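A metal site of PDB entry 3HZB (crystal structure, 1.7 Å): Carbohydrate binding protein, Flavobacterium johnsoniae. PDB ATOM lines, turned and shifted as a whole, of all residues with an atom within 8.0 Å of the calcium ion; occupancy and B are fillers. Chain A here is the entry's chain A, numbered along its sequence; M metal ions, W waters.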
ATOM      1  N   TYR A   6      14.609  -1.602  29.945  1.00  0.00           N
ATOM      2  CA  TYR A   6      13.326  -0.937  30.126  1.00  0.00           C
ATOM      3  C   TYR A   6      13.017   0.144  29.112  1.00  0.00           C
ATOM      4  O   TYR A   6      13.912   0.855  28.633  1.00  0.00           O
ATOM      5  CB  TYR A   6      13.259  -0.302  31.513  1.00  0.00           C
ATOM      6  CG  TYR A   6      13.504  -1.259  32.649  1.00  0.00           C
ATOM      7  CD1 TYR A   6      14.801  -1.672  32.978  1.00  0.00           C
ATOM      8  CD2 TYR A   6      12.453  -1.737  33.428  1.00  0.00           C
ATOM      9  CE1 TYR A   6      15.033  -2.537  34.044  1.00  0.00           C
ATOM     10  CE2 TYR A   6      12.671  -2.600  34.493  1.00  0.00           C
ATOM     11  CZ  TYR A   6      13.959  -2.994  34.803  1.00  0.00           C
ATOM     12  OH  TYR A   6      14.179  -3.850  35.851  1.00  0.00           O
ATOM     13  N   LYS A   7      11.728   0.281  28.822  1.00  0.00           N
ATOM     14  CA  LYS A   7      11.260   1.273  27.875  1.00  0.00           C
ATOM     15  C   LYS A   7      11.520   2.673  28.378  1.00  0.00           C
ATOM     16  O   LYS A   7      11.978   3.524  27.632  1.00  0.00           O
ATOM     17  CB  LYS A   7       9.757   1.109  27.624  1.00  0.00           C
ATOM     18  CG  LYS A   7       9.212   2.024  26.531  1.00  0.00           C
ATOM     19  CD  LYS A   7       7.694   1.902  26.415  1.00  0.00           C
ATOM     20  CE  LYS A   7       7.178   2.576  25.152  1.00  0.00           C
ATOM     21  NZ  LYS A   7       7.614   1.854  23.918  1.00  0.00           N
ATOM     22  N   ASP A   8      11.259   2.938  29.653  1.00  0.00           N
ATOM     23  CA  ASP A   8      11.470   4.279  30.175  1.00  0.00           C
ATOM     24  C   ASP A   8      12.646   4.392  31.131  1.00  0.00           C
ATOM     25  O   ASP A   8      13.215   3.392  31.554  1.00  0.00           O
ATOM     26  CB  ASP A   8      10.198   4.779  30.863  1.00  0.00           C
ATOM     27  CG  ASP A   8       8.977   4.679  29.975  1.00  0.00           C
ATOM     28  OD1 ASP A   8       9.062   5.132  28.806  1.00  0.00           O
ATOM     29  OD2 ASP A   8       7.940   4.163  30.444  1.00  0.00           O
ATOM     30  N   CYS A   9      13.010   5.629  31.463  1.00  0.00           N
ATOM     31  CA  CYS A   9      14.111   5.863  32.376  1.00  0.00           C
ATOM     32  C   CYS A   9      13.711   5.436  33.791  1.00  0.00           C
ATOM     33  O   CYS A   9      12.526   5.277  34.076  1.00  0.00           O
ATOM     34  CB  CYS A   9      14.520   7.342  32.323  1.00  0.00           C
ATOM     35  SG  CYS A   9      15.574   7.665  30.868  1.00  0.00           S
ATOM     36  N   THR A  12      11.517   1.690  34.518  1.00  0.00           N
ATOM     37  CA  THR A  12      10.069   1.618  34.458  1.00  0.00           C
ATOM     38  C   THR A  12       9.639   1.407  33.001  1.00  0.00           C
ATOM     39  O   THR A  12      10.456   1.562  32.091  1.00  0.00           O
ATOM     40  CB  THR A  12       9.408   2.898  35.006  1.00  0.00           C
ATOM     41  OG1 THR A  12       9.841   4.017  34.222  1.00  0.00           O
ATOM     42  CG2 THR A  12       9.812   3.123  36.460  1.00  0.00           C
ATOM     43  N   ASN A  35      12.606  -1.428  18.873  1.00  0.00           N
ATOM     44  CA  ASN A  35      13.796  -0.782  18.329  1.00  0.00           C
ATOM     45  C   ASN A  35      13.778   0.681  18.760  1.00  0.00           C
ATOM     46  O   ASN A  35      12.695   1.236  18.963  1.00  0.00           O
ATOM     47  CB  ASN A  35      13.753  -0.850  16.800  1.00  0.00           C
ATOM     48  CG  ASN A  35      14.967  -0.232  16.154  1.00  0.00           C
ATOM     49  OD1 ASN A  35      14.856   0.736  15.395  1.00  0.00           O
ATOM     50  ND2 ASN A  35      16.130  -0.790  16.446  1.00  0.00           N
ATOM     51  N   ASP A  36      14.952   1.295  18.881  1.00  0.00           N
ATOM     52  CA  ASP A  36      15.063   2.700  19.264  1.00  0.00           C
ATOM     53  C   ASP A  36      14.035   3.031  20.329  1.00  0.00           C
ATOM     54  O   ASP A  36      13.245   3.958  20.176  1.00  0.00           O
ATOM     55  CB  ASP A  36      14.813   3.598  18.039  1.00  0.00           C
ATOM     56  CG  ASP A  36      15.906   3.456  16.991  1.00  0.00           C
ATOM     57  OD1 ASP A  36      16.867   2.704  17.255  1.00  0.00           O
ATOM     58  OD2 ASP A  36      15.810   4.095  15.929  1.00  0.00           O
ATOM     59  N   ASP A  37      14.078   2.285  21.428  1.00  0.00           N
ATOM     60  CA  ASP A  37      13.089   2.478  22.474  1.00  0.00           C
ATOM     61  C   ASP A  37      13.622   2.316  23.901  1.00  0.00           C
ATOM     62  O   ASP A  37      13.050   2.865  24.829  1.00  0.00           O
ATOM     63  CB  ASP A  37      11.963   1.471  22.223  1.00  0.00           C
ATOM     64  CG  ASP A  37      10.723   1.772  23.036  1.00  0.00           C
ATOM     65  OD1 ASP A  37      10.277   0.862  23.759  1.00  0.00           O
ATOM     66  OD2 ASP A  37      10.201   2.904  22.932  1.00  0.00           O
ATOM     67  N   ILE A  38      14.694   1.555  24.090  1.00  0.00           N
ATOM     68  CA  ILE A  38      15.218   1.355  25.430  1.00  0.00           C
ATOM     69  C   ILE A  38      15.782   2.638  26.025  1.00  0.00           C
ATOM     70  O   ILE A  38      16.450   3.403  25.332  1.00  0.00           O
ATOM     71  CB  ILE A  38      16.319   0.265  25.424  1.00  0.00           C
ATOM     72  CG1 ILE A  38      15.694  -1.077  25.021  1.00  0.00           C
ATOM     73  CG2 ILE A  38      16.977   0.171  26.803  1.00  0.00           C
ATOM     74  CD1 ILE A  38      16.712  -2.132  24.658  1.00  0.00           C
ATOM     75  N   SER A  39      15.500   2.877  27.305  1.00  0.00           N
ATOM     76  CA  SER A  39      15.984   4.077  27.974  1.00  0.00           C
ATOM     77  C   SER A  39      16.786   3.836  29.251  1.00  0.00           C
ATOM     78  O   SER A  39      17.484   4.732  29.732  1.00  0.00           O
ATOM     79  CB  SER A  39      14.822   5.007  28.296  1.00  0.00           C
ATOM     80  OG  SER A  39      14.410   5.643  27.102  1.00  0.00           O
ATOM     81  N   SER A  40      16.672   2.647  29.828  1.00  0.00           N
ATOM     82  CA  SER A  40      17.437   2.305  31.032  1.00  0.00           C
ATOM     83  C   SER A  40      17.593   0.803  31.098  1.00  0.00           C
ATOM     84  O   SER A  40      16.859   0.063  30.430  1.00  0.00           O
ATOM     85  CB  SER A  40      16.751   2.835  32.295  1.00  0.00           C
ATOM     86  OG  SER A  40      15.512   2.197  32.531  1.00  0.00           O
ATOM     87  N   LEU A  71      19.778   6.475  29.702  1.00  0.00           N
ATOM     88  CA  LEU A  71      20.817   6.582  28.685  1.00  0.00           C
ATOM     89  C   LEU A  71      20.925   8.017  28.178  1.00  0.00           C
ATOM     90  O   LEU A  71      19.936   8.756  28.169  1.00  0.00           O
ATOM     91  CB  LEU A  71      20.502   5.629  27.532  1.00  0.00           C
ATOM     92  CG  LEU A  71      20.553   4.140  27.897  1.00  0.00           C
ATOM     93  CD1 LEU A  71      19.939   3.297  26.769  1.00  0.00           C
ATOM     94  CD2 LEU A  71      21.998   3.724  28.158  1.00  0.00           C
ATOM     95  N   ASN A  76      19.928   6.936  24.144  1.00  0.00           N
ATOM     96  CA  ASN A  76      18.520   6.807  24.496  1.00  0.00           C
ATOM     97  C   ASN A  76      17.649   6.675  23.263  1.00  0.00           C
ATOM     98  O   ASN A  76      17.773   7.450  22.321  1.00  0.00           O
ATOM     99  CB  ASN A  76      18.057   8.019  25.311  1.00  0.00           C
ATOM    100  CG  ASN A  76      16.606   7.914  25.729  1.00  0.00           C
ATOM    101  OD1 ASN A  76      16.213   6.955  26.378  1.00  0.00           O
ATOM    102  ND2 ASN A  76      15.799   8.887  25.333  1.00  0.00           N
ATOM    103  N   ASP A  77      16.766   5.671  23.264  1.00  0.00           N
ATOM    104  CA  ASP A  77      15.878   5.418  22.129  1.00  0.00           C
ATOM    105  C   ASP A  77      16.632   5.220  20.824  1.00  0.00           C
ATOM    106  O   ASP A  77      16.175   5.644  19.770  1.00  0.00           O
ATOM    107  CB  ASP A  77      14.882   6.573  21.957  1.00  0.00           C
ATOM    108  CG  ASP A  77      13.943   6.696  23.121  1.00  0.00           C
ATOM    109  OD1 ASP A  77      13.804   5.686  23.824  1.00  0.00           O
ATOM    110  OD2 ASP A  77      13.353   7.773  23.324  1.00  0.00           O
ATOM    111  N   LYS A  78      17.803   4.593  20.907  1.00  0.00           N
ATOM    112  CA  LYS A  78      18.622   4.364  19.719  1.00  0.00           C
ATOM    113  C   LYS A  78      19.145   2.931  19.585  1.00  0.00           C
ATOM    114  O   LYS A  78      19.643   2.548  18.531  1.00  0.00           O
ATOM    115  CB  LYS A  78      19.819   5.315  19.732  1.00  0.00           C
ATOM    116  CG  LYS A  78      19.459   6.782  19.595  1.00  0.00           C
ATOM    117  CD  LYS A  78      18.900   7.086  18.217  1.00  0.00           C
ATOM    118  CE  LYS A  78      18.557   8.556  18.065  1.00  0.00           C
ATOM    119  NZ  LYS A  78      17.960   8.823  16.723  1.00  0.00           N
HETATM  120 CA    CA M   1      12.366   5.061  25.783  1.00  0.00          CA
HETATM  121  O   HOH W   1      10.300   4.997  24.271  1.00  0.00           O
HETATM  122  O   HOH W   2      10.647   6.665  27.383  1.00  0.00           O
HETATM  123  O   HOH W   3      12.347   7.751  25.742  1.00  0.00           O
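N of Ser 39 sits at hydrogen-bond distance from O of Tyr 6, 2.9 Å away.
O of Ser 39 lies within hydrogen-bond range of N of Leu 71, 2.9 Å away.
N of Asp 77 lies within hydrogen-bond range of O of Ile 38, at 3.1 Å.
The side-chain carboxylate (OD2) of Asp 77 is in hydrogen-bond range of the side-chain amide nitrogen (ND2) of Asn 76, 3.4 Å away.
Within 4 Å of the calcium ion: Lys 7, Asp 37, Ser 39 and Asp 77.
The calcium ion is bound by the backbone carbonyl oxygen (O) of Lys 7 (2.4 Å), the backbone carbonyl oxygen (O) of Asp 37 (2.5 Å), the side-chain hydroxyl (OG) of Ser 39 (2.5 Å), the side-chain carboxylate (OD1) of Asp 77 (2.5 Å), water W1 (2.6 Å), water W3 (2.7 Å) and water W2 (2.8 Å).
The calcium ion has seven donor atoms within binding distance.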
